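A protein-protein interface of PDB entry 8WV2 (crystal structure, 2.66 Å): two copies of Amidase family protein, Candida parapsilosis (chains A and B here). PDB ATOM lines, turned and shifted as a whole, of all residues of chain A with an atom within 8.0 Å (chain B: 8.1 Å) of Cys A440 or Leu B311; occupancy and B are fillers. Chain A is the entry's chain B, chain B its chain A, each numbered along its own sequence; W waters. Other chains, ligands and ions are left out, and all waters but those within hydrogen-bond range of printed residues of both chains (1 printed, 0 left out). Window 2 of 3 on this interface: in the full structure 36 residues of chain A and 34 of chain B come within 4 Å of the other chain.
The side-chain sulfur of Cys A440 sits at hydrogen-bond distance from the backbone carbonyl oxygen of Leu B311 (3.6 Å). The backbone carbonyl oxygen (O) of Pro B314 is in hydrogen-bond range of the guanidinium group (NE) of Arg A536 (3.1 Å).
The backbone carbonyl oxygen (O) of Cys A440 lies within hydrogen-bond range of the side-chain hydroxyl (OG1) of Thr A443 (2.9 Å). The side-chain sulfur of Cys A440 is in hydrogen-bond range of the backbone carbonyl oxygen of Leu A436. OD1 of Asp B313 is in hydrogen-bond range of OG1 of Thr B315 (2.6 Å).
Ile B312 touches Lys A433 (O to CG, 3.6 Å). Pro B314 touches Lys A433. O of Trp B310 touches CD2 of Leu A436, 3.3 Å away. Leu B311 touches Leu A436 (C to CD2, 3.5 Å). Ile B312 touches Leu A436. Leu A436 touches Pro B314 (CD2 to N, 3.8 Å). Arg A536 touches Thr B315.
Of the printed residues of chain B, Lys A433 touches Ile B312 (3.6 Å) and Pro B314 (3.9 Å). Of the printed residues of chain B, Leu A436 touches Trp B310 (3.3 Å), Leu B311 (3.5 Å), Ile B312 (3.6 Å) and Pro B314 (3.8 Å). Cys A440 touches just one residue of chain B: Leu B311. Asn A448 touches none of the printed residues of chain B. Leu B311 touches just these residues of chain A: Leu A436 and Cys A440. Of the printed residues of chain A, Pro B314 touches Lys A433 (3.9 Å), Leu A436 (3.8 Å) and Arg A536 (3.1 Å).
Of the 22 printed residues of chain A, 4 touch a printed residue of chain B. Of the 13 printed residues of chain B, 5 touch a printed residue of chain A. Hydrophobic or aromatic side chains of chain B that line the printed part of chain A: Pro B314. Among the printed residues, 9 pairs touch across the chains. Among the printed residues, no Asp or Glu carboxylate lies within 4 Å of a Lys or Arg side-chain nitrogen of the other chain.
No position is printed for both chains. Of the 9 pairs that touch across the chains among the printed residues, none has its exchanged pair printed and touching as well.
Water W1 lies within hydrogen-bond range of NH2 of Arg A536 (2.5 Å) and O of Thr B315 (3.1 Å).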
ATOM      1  N   ARG A 330     -35.224 -15.886  21.939  1.00  0.00           N
ATOM      2  CA  ARG A 330     -34.839 -15.745  23.345  1.00  0.00           C
ATOM      3  C   ARG A 330     -34.258 -14.325  23.417  1.00  0.00           C
ATOM      4  O   ARG A 330     -33.282 -14.052  22.754  1.00  0.00           O
ATOM      5  CB  ARG A 330     -33.882 -16.817  23.814  1.00  0.00           C
ATOM      6  CG  ARG A 330     -34.515 -18.161  24.118  1.00  0.00           C
ATOM      7  CD  ARG A 330     -33.467 -19.111  24.659  1.00  0.00           C
ATOM      8  NE  ARG A 330     -32.566 -18.412  25.560  1.00  0.00           N
ATOM      9  CZ  ARG A 330     -32.702 -18.378  26.875  1.00  0.00           C
ATOM     10  NH1 ARG A 330     -33.689 -19.017  27.466  1.00  0.00           N
ATOM     11  NH2 ARG A 330     -31.847 -17.704  27.604  1.00  0.00           N
ATOM     12  N   PHE A 368     -31.398  -9.168  31.717  1.00  0.00           N
ATOM     13  CA  PHE A 368     -30.004  -9.152  31.286  1.00  0.00           C
ATOM     14  C   PHE A 368     -29.201  -8.233  32.197  1.00  0.00           C
ATOM     15  O   PHE A 368     -29.457  -7.025  32.249  1.00  0.00           O
ATOM     16  CB  PHE A 368     -29.889  -8.710  29.829  1.00  0.00           C
ATOM     17  CG  PHE A 368     -28.501  -8.831  29.275  1.00  0.00           C
ATOM     18  CD1 PHE A 368     -28.044 -10.048  28.794  1.00  0.00           C
ATOM     19  CD2 PHE A 368     -27.662  -7.731  29.211  1.00  0.00           C
ATOM     20  CE1 PHE A 368     -26.770 -10.169  28.280  1.00  0.00           C
ATOM     21  CE2 PHE A 368     -26.382  -7.849  28.694  1.00  0.00           C
ATOM     22  CZ  PHE A 368     -25.940  -9.068  28.226  1.00  0.00           C
ATOM     23  N   LYS A 433     -13.827 -10.755  24.994  1.00  0.00           N
ATOM     24  CA  LYS A 433     -13.932 -12.193  25.212  1.00  0.00           C
ATOM     25  C   LYS A 433     -14.704 -12.501  26.487  1.00  0.00           C
ATOM     26  O   LYS A 433     -15.538 -13.412  26.508  1.00  0.00           O
ATOM     27  CB  LYS A 433     -12.535 -12.816  25.256  1.00  0.00           C
ATOM     28  CG  LYS A 433     -12.538 -14.292  24.922  1.00  0.00           C
ATOM     29  CD  LYS A 433     -11.145 -14.844  24.811  1.00  0.00           C
ATOM     30  CE  LYS A 433     -11.174 -16.243  24.223  1.00  0.00           C
ATOM     31  NZ  LYS A 433      -9.829 -16.898  24.204  1.00  0.00           N
ATOM     32  N   GLU A 434     -14.427 -11.764  27.564  1.00  0.00           N
ATOM     33  CA  GLU A 434     -15.195 -11.952  28.790  1.00  0.00           C
ATOM     34  C   GLU A 434     -16.677 -11.675  28.565  1.00  0.00           C
ATOM     35  O   GLU A 434     -17.533 -12.430  29.036  1.00  0.00           O
ATOM     36  CB  GLU A 434     -14.650 -11.060  29.903  1.00  0.00           C
ATOM     37  CG  GLU A 434     -13.330 -11.530  30.478  1.00  0.00           C
ATOM     38  CD  GLU A 434     -12.588 -10.421  31.197  1.00  0.00           C
ATOM     39  OE1 GLU A 434     -13.239  -9.450  31.651  1.00  0.00           O
ATOM     40  OE2 GLU A 434     -11.348 -10.522  31.305  1.00  0.00           O
ATOM     41  N   PHE A 435     -17.001 -10.619  27.816  1.00  0.00           N
ATOM     42  CA  PHE A 435     -18.404 -10.266  27.655  1.00  0.00           C
ATOM     43  C   PHE A 435     -19.136 -11.345  26.877  1.00  0.00           C
ATOM     44  O   PHE A 435     -20.284 -11.679  27.191  1.00  0.00           O
ATOM     45  CB  PHE A 435     -18.540  -8.920  26.939  1.00  0.00           C
ATOM     46  CG  PHE A 435     -19.902  -8.298  27.073  1.00  0.00           C
ATOM     47  CD1 PHE A 435     -20.125  -7.283  27.996  1.00  0.00           C
ATOM     48  CD2 PHE A 435     -20.956  -8.715  26.273  1.00  0.00           C
ATOM     49  CE1 PHE A 435     -21.377  -6.706  28.131  1.00  0.00           C
ATOM     50  CE2 PHE A 435     -22.212  -8.147  26.402  1.00  0.00           C
ATOM     51  CZ  PHE A 435     -22.423  -7.138  27.332  1.00  0.00           C
ATOM     52  N   LEU A 436     -18.481 -11.907  25.863  1.00  0.00           N
ATOM     53  CA  LEU A 436     -19.087 -12.999  25.118  1.00  0.00           C
ATOM     54  C   LEU A 436     -19.424 -14.148  26.060  1.00  0.00           C
ATOM     55  O   LEU A 436     -20.504 -14.741  25.964  1.00  0.00           O
ATOM     56  CB  LEU A 436     -18.144 -13.446  24.002  1.00  0.00           C
ATOM     57  CG  LEU A 436     -18.684 -14.502  23.042  1.00  0.00           C
ATOM     58  CD1 LEU A 436     -20.026 -14.040  22.476  1.00  0.00           C
ATOM     59  CD2 LEU A 436     -17.689 -14.820  21.924  1.00  0.00           C
ATOM     60  N   LYS A 437     -18.514 -14.453  26.994  1.00  0.00           N
ATOM     61  CA  LYS A 437     -18.777 -15.469  28.006  1.00  0.00           C
ATOM     62  C   LYS A 437     -19.992 -15.089  28.829  1.00  0.00           C
ATOM     63  O   LYS A 437     -20.830 -15.939  29.148  1.00  0.00           O
ATOM     64  CB  LYS A 437     -17.544 -15.636  28.905  1.00  0.00           C
ATOM     65  CG  LYS A 437     -17.589 -16.752  29.959  1.00  0.00           C
ATOM     66  CD  LYS A 437     -16.287 -16.725  30.785  1.00  0.00           C
ATOM     67  CE  LYS A 437     -16.137 -15.417  31.597  1.00  0.00           C
ATOM     68  NZ  LYS A 437     -14.905 -15.390  32.462  1.00  0.00           N
ATOM     69  N   HIS A 438     -20.120 -13.804  29.157  1.00  0.00           N
ATOM     70  CA  HIS A 438     -21.305 -13.335  29.865  1.00  0.00           C
ATOM     71  C   HIS A 438     -22.572 -13.567  29.042  1.00  0.00           C
ATOM     72  O   HIS A 438     -23.550 -14.137  29.538  1.00  0.00           O
ATOM     73  CB  HIS A 438     -21.132 -11.858  30.224  1.00  0.00           C
ATOM     74  CG  HIS A 438     -22.295 -11.275  30.962  1.00  0.00           C
ATOM     75  ND1 HIS A 438     -22.593 -11.606  32.266  1.00  0.00           N
ATOM     76  CD2 HIS A 438     -23.239 -10.383  30.576  1.00  0.00           C
ATOM     77  CE1 HIS A 438     -23.668 -10.942  32.654  1.00  0.00           C
ATOM     78  NE2 HIS A 438     -24.081 -10.195  31.646  1.00  0.00           N
ATOM     79  N   TRP A 439     -22.561 -13.143  27.773  1.00  0.00           N
ATOM     80  CA  TRP A 439     -23.728 -13.310  26.906  1.00  0.00           C
ATOM     81  C   TRP A 439     -24.135 -14.776  26.796  1.00  0.00           C
ATOM     82  O   TRP A 439     -25.320 -15.113  26.898  1.00  0.00           O
ATOM     83  CB  TRP A 439     -23.432 -12.724  25.523  1.00  0.00           C
ATOM     84  CG  TRP A 439     -24.571 -12.763  24.530  1.00  0.00           C
ATOM     85  CD1 TRP A 439     -25.079 -13.866  23.887  1.00  0.00           C
ATOM     86  CD2 TRP A 439     -25.320 -11.643  24.042  1.00  0.00           C
ATOM     87  NE1 TRP A 439     -26.102 -13.496  23.042  1.00  0.00           N
ATOM     88  CE2 TRP A 439     -26.270 -12.139  23.120  1.00  0.00           C
ATOM     89  CE3 TRP A 439     -25.285 -10.268  24.303  1.00  0.00           C
ATOM     90  CZ2 TRP A 439     -27.168 -11.309  22.454  1.00  0.00           C
ATOM     91  CZ3 TRP A 439     -26.183  -9.445  23.646  1.00  0.00           C
ATOM     92  CH2 TRP A 439     -27.112  -9.967  22.732  1.00  0.00           C
ATOM     93  N   CYS A 440     -23.163 -15.664  26.582  1.00  0.00           N
ATOM     94  CA  CYS A 440     -23.471 -17.081  26.435  1.00  0.00           C
ATOM     95  C   CYS A 440     -23.947 -17.721  27.735  1.00  0.00           C
ATOM     96  O   CYS A 440     -24.580 -18.775  27.688  1.00  0.00           O
ATOM     97  CB  CYS A 440     -22.251 -17.821  25.890  1.00  0.00           C
ATOM     98  SG  CYS A 440     -21.830 -17.415  24.168  1.00  0.00           S
ATOM     99  N   SER A 441     -23.680 -17.107  28.889  1.00  0.00           N
ATOM    100  CA  SER A 441     -24.211 -17.625  30.146  1.00  0.00           C
ATOM    101  C   SER A 441     -25.731 -17.574  30.201  1.00  0.00           C
ATOM    102  O   SER A 441     -26.321 -18.161  31.108  1.00  0.00           O
ATOM    103  CB  SER A 441     -23.616 -16.860  31.325  1.00  0.00           C
ATOM    104  OG  SER A 441     -24.413 -15.723  31.641  1.00  0.00           O
ATOM    105  N   TYR A 442     -26.373 -16.871  29.272  1.00  0.00           N
ATOM    106  CA  TYR A 442     -27.825 -16.818  29.172  1.00  0.00           C
ATOM    107  C   TYR A 442     -28.404 -17.886  28.257  1.00  0.00           C
ATOM    108  O   TYR A 442     -29.624 -17.939  28.102  1.00  0.00           O
ATOM    109  CB  TYR A 442     -28.269 -15.433  28.693  1.00  0.00           C
ATOM    110  CG  TYR A 442     -28.086 -14.392  29.764  1.00  0.00           C
ATOM    111  CD1 TYR A 442     -29.079 -14.165  30.705  1.00  0.00           C
ATOM    112  CD2 TYR A 442     -26.902 -13.675  29.867  1.00  0.00           C
ATOM    113  CE1 TYR A 442     -28.910 -13.235  31.705  1.00  0.00           C
ATOM    114  CE2 TYR A 442     -26.722 -12.738  30.868  1.00  0.00           C
ATOM    115  CZ  TYR A 442     -27.730 -12.524  31.785  1.00  0.00           C
ATOM    116  OH  TYR A 442     -27.558 -11.597  32.786  1.00  0.00           O
ATOM    117  N   THR A 443     -27.568 -18.717  27.633  1.00  0.00           N
ATOM    118  CA  THR A 443     -28.073 -19.840  26.850  1.00  0.00           C
ATOM    119  C   THR A 443     -28.880 -20.778  27.744  1.00  0.00           C
ATOM    120  O   THR A 443     -28.535 -20.995  28.907  1.00  0.00           O
ATOM    121  CB  THR A 443     -26.911 -20.587  26.195  1.00  0.00           C
ATOM    122  OG1 THR A 443     -26.156 -19.675  25.393  1.00  0.00           O
ATOM    123  CG2 THR A 443     -27.431 -21.669  25.286  1.00  0.00           C
ATOM    124  N   ASP A 444     -29.983 -21.307  27.209  1.00  0.00           N
ATOM    125  CA  ASP A 444     -30.882 -22.157  27.982  1.00  0.00           C
ATOM    126  C   ASP A 444     -30.434 -23.622  27.974  1.00  0.00           C
ATOM    127  O   ASP A 444     -29.387 -23.985  27.430  1.00  0.00           O
ATOM    128  CB  ASP A 444     -32.327 -22.003  27.498  1.00  0.00           C
ATOM    129  CG  ASP A 444     -32.546 -22.511  26.086  1.00  0.00           C
ATOM    130  OD1 ASP A 444     -31.597 -23.036  25.467  1.00  0.00           O
ATOM    131  OD2 ASP A 444     -33.690 -22.389  25.596  1.00  0.00           O
ATOM    132  N   GLY A 447     -29.611 -25.246  24.683  1.00  0.00           N
ATOM    133  CA  GLY A 447     -28.578 -24.659  23.857  1.00  0.00           C
ATOM    134  C   GLY A 447     -29.027 -23.528  22.959  1.00  0.00           C
ATOM    135  O   GLY A 447     -28.330 -23.216  21.986  1.00  0.00           O
ATOM    136  N   ASN A 448     -30.159 -22.895  23.251  1.00  0.00           N
ATOM    137  CA  ASN A 448     -30.623 -21.764  22.458  1.00  0.00           C
ATOM    138  C   ASN A 448     -29.969 -20.502  23.000  1.00  0.00           C
ATOM    139  O   ASN A 448     -30.202 -20.128  24.155  1.00  0.00           O
ATOM    140  CB  ASN A 448     -32.142 -21.630  22.510  1.00  0.00           C
ATOM    141  CG  ASN A 448     -32.861 -22.893  22.084  1.00  0.00           C
ATOM    142  OD1 ASN A 448     -33.726 -23.390  22.803  1.00  0.00           O
ATOM    143  ND2 ASN A 448     -32.497 -23.427  20.923  1.00  0.00           N
ATOM    144  N   VAL A 449     -29.146 -19.852  22.175  1.00  0.00           N
ATOM    145  CA  VAL A 449     -28.468 -18.646  22.626  1.00  0.00           C
ATOM    146  C   VAL A 449     -29.462 -17.496  22.705  1.00  0.00           C
ATOM    147  O   VAL A 449     -30.548 -17.530  22.117  1.00  0.00           O
ATOM    148  CB  VAL A 449     -27.285 -18.287  21.713  1.00  0.00           C
ATOM    149  CG1 VAL A 449     -26.431 -19.523  21.429  1.00  0.00           C
ATOM    150  CG2 VAL A 449     -27.784 -17.636  20.430  1.00  0.00           C
ATOM    151  N   LEU A 450     -29.095 -16.476  23.481  1.00  0.00           N
ATOM    152  CA  LEU A 450     -29.802 -15.204  23.419  1.00  0.00           C
ATOM    153  C   LEU A 450     -29.731 -14.641  22.006  1.00  0.00           C
ATOM    154  O   LEU A 450     -28.643 -14.492  21.439  1.00  0.00           O
ATOM    155  CB  LEU A 450     -29.196 -14.209  24.407  1.00  0.00           C
ATOM    156  CG  LEU A 450     -29.900 -13.941  25.737  1.00  0.00           C
ATOM    157  CD1 LEU A 450     -29.238 -12.766  26.444  1.00  0.00           C
ATOM    158  CD2 LEU A 450     -31.367 -13.663  25.519  1.00  0.00           C
ATOM    159  N   TYR A 482     -20.776  -4.726  18.651  1.00  0.00           N
ATOM    160  CA  TYR A 482     -22.023  -5.454  18.429  1.00  0.00           C
ATOM    161  C   TYR A 482     -22.969  -4.611  17.576  1.00  0.00           C
ATOM    162  O   TYR A 482     -23.033  -3.393  17.750  1.00  0.00           O
ATOM    163  CB  TYR A 482     -22.716  -5.779  19.751  1.00  0.00           C
ATOM    164  CG  TYR A 482     -22.131  -6.914  20.542  1.00  0.00           C
ATOM    165  CD1 TYR A 482     -20.922  -7.509  20.174  1.00  0.00           C
ATOM    166  CD2 TYR A 482     -22.800  -7.417  21.655  1.00  0.00           C
ATOM    167  CE1 TYR A 482     -20.392  -8.557  20.897  1.00  0.00           C
ATOM    168  CE2 TYR A 482     -22.269  -8.478  22.389  1.00  0.00           C
ATOM    169  CZ  TYR A 482     -21.070  -9.037  22.001  1.00  0.00           C
ATOM    170  OH  TYR A 482     -20.538 -10.084  22.717  1.00  0.00           O
ATOM    171  N   LEU A 535     -25.353 -10.177  18.843  1.00  0.00           N
ATOM    172  CA  LEU A 535     -23.979 -10.601  18.640  1.00  0.00           C
ATOM    173  C   LEU A 535     -23.509 -10.199  17.244  1.00  0.00           C
ATOM    174  O   LEU A 535     -24.309  -9.888  16.354  1.00  0.00           O
ATOM    175  CB  LEU A 535     -23.840 -12.114  18.830  1.00  0.00           C
ATOM    176  CG  LEU A 535     -24.121 -12.610  20.254  1.00  0.00           C
ATOM    177  CD1 LEU A 535     -24.016 -14.134  20.387  1.00  0.00           C
ATOM    178  CD2 LEU A 535     -23.203 -11.905  21.255  1.00  0.00           C
ATOM    179  N   ARG A 536     -22.192 -10.219  17.063  1.00  0.00           N
ATOM    180  CA  ARG A 536     -21.584  -9.747  15.829  1.00  0.00           C
ATOM    181  C   ARG A 536     -22.181 -10.440  14.612  1.00  0.00           C
ATOM    182  O   ARG A 536     -22.361 -11.659  14.599  1.00  0.00           O
ATOM    183  CB  ARG A 536     -20.071  -9.968  15.882  1.00  0.00           C
ATOM    184  CG  ARG A 536     -19.426  -9.270  17.068  1.00  0.00           C
ATOM    185  CD  ARG A 536     -18.247  -8.384  16.675  1.00  0.00           C
ATOM    186  NE  ARG A 536     -17.213  -9.102  15.940  1.00  0.00           N
ATOM    187  CZ  ARG A 536     -16.681  -8.673  14.800  1.00  0.00           C
ATOM    188  NH1 ARG A 536     -17.079  -7.512  14.293  1.00  0.00           N
ATOM    189  NH2 ARG A 536     -15.735  -9.386  14.184  1.00  0.00           N
ATOM    190  N   THR A 538     -25.180 -10.408  13.496  1.00  0.00           N
ATOM    191  CA  THR A 538     -26.591 -10.767  13.613  1.00  0.00           C
ATOM    192  C   THR A 538     -27.511  -9.567  13.374  1.00  0.00           C
ATOM    193  O   THR A 538     -28.604  -9.503  13.943  1.00  0.00           O
ATOM    194  CB  THR A 538     -26.881 -11.403  14.978  1.00  0.00           C
ATOM    195  OG1 THR A 538     -26.752 -10.417  16.015  1.00  0.00           O
ATOM    196  CG2 THR A 538     -25.895 -12.556  15.256  1.00  0.00           C
ATOM    197  N   ILE B 180     -11.298 -26.980  21.267  1.00  0.00           N
ATOM    198  CA  ILE B 180     -12.282 -27.318  20.244  1.00  0.00           C
ATOM    199  C   ILE B 180     -11.935 -28.656  19.608  1.00  0.00           C
ATOM    200  O   ILE B 180     -12.796 -29.527  19.436  1.00  0.00           O
ATOM    201  CB  ILE B 180     -12.375 -26.210  19.180  1.00  0.00           C
ATOM    202  CG1 ILE B 180     -13.108 -24.985  19.723  1.00  0.00           C
ATOM    203  CG2 ILE B 180     -13.088 -26.753  17.950  1.00  0.00           C
ATOM    204  CD1 ILE B 180     -13.036 -23.791  18.799  1.00  0.00           C
ATOM    205  N   ALA B 307     -17.750 -25.952  14.714  1.00  0.00           N
ATOM    206  CA  ALA B 307     -17.955 -25.857  16.153  1.00  0.00           C
ATOM    207  C   ALA B 307     -18.331 -24.450  16.614  1.00  0.00           C
ATOM    208  O   ALA B 307     -18.468 -24.232  17.821  1.00  0.00           O
ATOM    209  CB  ALA B 307     -16.698 -26.326  16.887  1.00  0.00           C
ATOM    210  N   LYS B 308     -18.508 -23.504  15.685  1.00  0.00           N
ATOM    211  CA  LYS B 308     -18.903 -22.114  15.921  1.00  0.00           C
ATOM    212  C   LYS B 308     -17.952 -21.406  16.885  1.00  0.00           C
ATOM    213  O   LYS B 308     -18.383 -20.916  17.939  1.00  0.00           O
ATOM    214  CB  LYS B 308     -20.336 -22.035  16.451  1.00  0.00           C
ATOM    215  CG  LYS B 308     -21.398 -22.622  15.531  1.00  0.00           C
ATOM    216  CD  LYS B 308     -22.743 -22.729  16.245  1.00  0.00           C
ATOM    217  CE  LYS B 308     -23.699 -23.611  15.474  1.00  0.00           C
ATOM    218  NZ  LYS B 308     -24.459 -22.815  14.487  1.00  0.00           N
ATOM    219  N   PRO B 309     -16.662 -21.299  16.546  1.00  0.00           N
ATOM    220  CA  PRO B 309     -15.713 -20.682  17.481  1.00  0.00           C
ATOM    221  C   PRO B 309     -15.979 -19.204  17.726  1.00  0.00           C
ATOM    222  O   PRO B 309     -15.394 -18.634  18.665  1.00  0.00           O
ATOM    223  CB  PRO B 309     -14.358 -20.905  16.797  1.00  0.00           C
ATOM    224  CG  PRO B 309     -14.688 -21.007  15.343  1.00  0.00           C
ATOM    225  CD  PRO B 309     -16.028 -21.662  15.266  1.00  0.00           C
ATOM    226  N   TRP B 310     -16.834 -18.562  16.918  1.00  0.00           N
ATOM    227  CA  TRP B 310     -17.219 -17.180  17.194  1.00  0.00           C
ATOM    228  C   TRP B 310     -18.073 -17.058  18.450  1.00  0.00           C
ATOM    229  O   TRP B 310     -18.350 -15.933  18.886  1.00  0.00           O
ATOM    230  CB  TRP B 310     -17.964 -16.576  16.003  1.00  0.00           C
ATOM    231  CG  TRP B 310     -19.125 -17.397  15.537  1.00  0.00           C
ATOM    232  CD1 TRP B 310     -20.400 -17.351  16.006  1.00  0.00           C
ATOM    233  CD2 TRP B 310     -19.114 -18.380  14.495  1.00  0.00           C
ATOM    234  NE1 TRP B 310     -21.191 -18.255  15.327  1.00  0.00           N
ATOM    235  CE2 TRP B 310     -20.421 -18.900  14.397  1.00  0.00           C
ATOM    236  CE3 TRP B 310     -18.121 -18.881  13.646  1.00  0.00           C
ATOM    237  CZ2 TRP B 310     -20.763 -19.892  13.481  1.00  0.00           C
ATOM    238  CZ3 TRP B 310     -18.469 -19.868  12.731  1.00  0.00           C
ATOM    239  CH2 TRP B 310     -19.777 -20.361  12.660  1.00  0.00           C
ATOM    240  N   LEU B 311     -18.517 -18.168  19.025  1.00  0.00           N
ATOM    241  CA  LEU B 311     -19.192 -18.143  20.313  1.00  0.00           C
ATOM    242  C   LEU B 311     -18.215 -18.253  21.474  1.00  0.00           C
ATOM    243  O   LEU B 311     -18.644 -18.204  22.633  1.00  0.00           O
ATOM    244  CB  LEU B 311     -20.234 -19.263  20.374  1.00  0.00           C
ATOM    245  CG  LEU B 311     -21.334 -19.079  19.317  1.00  0.00           C
ATOM    246  CD1 LEU B 311     -22.384 -20.190  19.355  1.00  0.00           C
ATOM    247  CD2 LEU B 311     -21.997 -17.682  19.431  1.00  0.00           C
ATOM    248  N   ILE B 312     -16.917 -18.385  21.177  1.00  0.00           N
ATOM    249  CA  ILE B 312     -15.857 -18.335  22.173  1.00  0.00           C
ATOM    250  C   ILE B 312     -14.910 -17.173  21.927  1.00  0.00           C
ATOM    251  O   ILE B 312     -14.538 -16.454  22.864  1.00  0.00           O
ATOM    252  CB  ILE B 312     -15.059 -19.661  22.192  1.00  0.00           C
ATOM    253  CG1 ILE B 312     -15.994 -20.874  22.238  1.00  0.00           C
ATOM    254  CG2 ILE B 312     -14.051 -19.662  23.331  1.00  0.00           C
ATOM    255  CD1 ILE B 312     -16.797 -21.006  23.533  1.00  0.00           C
ATOM    256  N   ASP B 313     -14.539 -16.950  20.668  1.00  0.00           N
ATOM    257  CA  ASP B 313     -13.613 -15.897  20.279  1.00  0.00           C
ATOM    258  C   ASP B 313     -14.361 -14.860  19.447  1.00  0.00           C
ATOM    259  O   ASP B 313     -14.691 -15.133  18.280  1.00  0.00           O
ATOM    260  CB  ASP B 313     -12.448 -16.504  19.487  1.00  0.00           C
ATOM    261  CG  ASP B 313     -11.354 -15.509  19.189  1.00  0.00           C
ATOM    262  OD1 ASP B 313     -11.586 -14.284  19.301  1.00  0.00           O
ATOM    263  OD2 ASP B 313     -10.251 -15.952  18.816  1.00  0.00           O
ATOM    264  N   PRO B 314     -14.628 -13.662  19.973  1.00  0.00           N
ATOM    265  CA  PRO B 314     -15.477 -12.705  19.252  1.00  0.00           C
ATOM    266  C   PRO B 314     -14.785 -12.008  18.095  1.00  0.00           C
ATOM    267  O   PRO B 314     -15.428 -11.192  17.419  1.00  0.00           O
ATOM    268  CB  PRO B 314     -15.861 -11.699  20.342  1.00  0.00           C
ATOM    269  CG  PRO B 314     -14.710 -11.720  21.293  1.00  0.00           C
ATOM    270  CD  PRO B 314     -14.128 -13.119  21.249  1.00  0.00           C
ATOM    271  N   THR B 315     -13.508 -12.303  17.836  1.00  0.00           N
ATOM    272  CA  THR B 315     -12.861 -11.750  16.656  1.00  0.00           C
ATOM    273  C   THR B 315     -13.237 -12.495  15.387  1.00  0.00           C
ATOM    274  O   THR B 315     -12.818 -12.086  14.304  1.00  0.00           O
ATOM    275  CB  THR B 315     -11.325 -11.755  16.809  1.00  0.00           C
ATOM    276  OG1 THR B 315     -10.874 -13.079  17.104  1.00  0.00           O
ATOM    277  CG2 THR B 315     -10.876 -10.825  17.919  1.00  0.00           C
ATOM    278  N   LEU B 316     -13.999 -13.578  15.488  1.00  0.00           N
ATOM    279  CA  LEU B 316     -14.247 -14.458  14.355  1.00  0.00           C
ATOM    280  C   LEU B 316     -15.603 -14.168  13.707  1.00  0.00           C
ATOM    281  O   LEU B 316     -16.524 -13.655  14.348  1.00  0.00           O
ATOM    282  CB  LEU B 316     -14.169 -15.931  14.788  1.00  0.00           C
ATOM    283  CG  LEU B 316     -12.898 -16.401  15.515  1.00  0.00           C
ATOM    284  CD1 LEU B 316     -12.949 -17.890  15.750  1.00  0.00           C
ATOM    285  CD2 LEU B 316     -11.620 -16.047  14.763  1.00  0.00           C
ATOM    286  N   VAL B 317     -15.715 -14.496  12.420  1.00  0.00           N
ATOM    287  CA  VAL B 317     -16.929 -14.218  11.656  1.00  0.00           C
ATOM    288  C   VAL B 317     -17.708 -15.516  11.475  1.00  0.00           C
ATOM    289  O   VAL B 317     -17.105 -16.572  11.225  1.00  0.00           O
ATOM    290  CB  VAL B 317     -16.601 -13.543  10.316  1.00  0.00           C
ATOM    291  CG1 VAL B 317     -15.577 -12.442  10.529  1.00  0.00           C
ATOM    292  CG2 VAL B 317     -16.101 -14.545   9.295  1.00  0.00           C
ATOM    293  N   PRO B 318     -19.035 -15.497  11.614  1.00  0.00           N
ATOM    294  CA  PRO B 318     -19.817 -16.732  11.428  1.00  0.00           C
ATOM    295  C   PRO B 318     -19.984 -17.086   9.956  1.00  0.00           C
ATOM    296  O   PRO B 318     -21.075 -17.067   9.400  1.00  0.00           O
ATOM    297  CB  PRO B 318     -21.150 -16.383  12.099  1.00  0.00           C
ATOM    298  CG  PRO B 318     -21.283 -14.918  11.906  1.00  0.00           C
ATOM    299  CD  PRO B 318     -19.895 -14.336  11.892  1.00  0.00           C
HETATM  300  O   HOH W   1     -14.184 -10.116  12.342  1.00  0.00           O
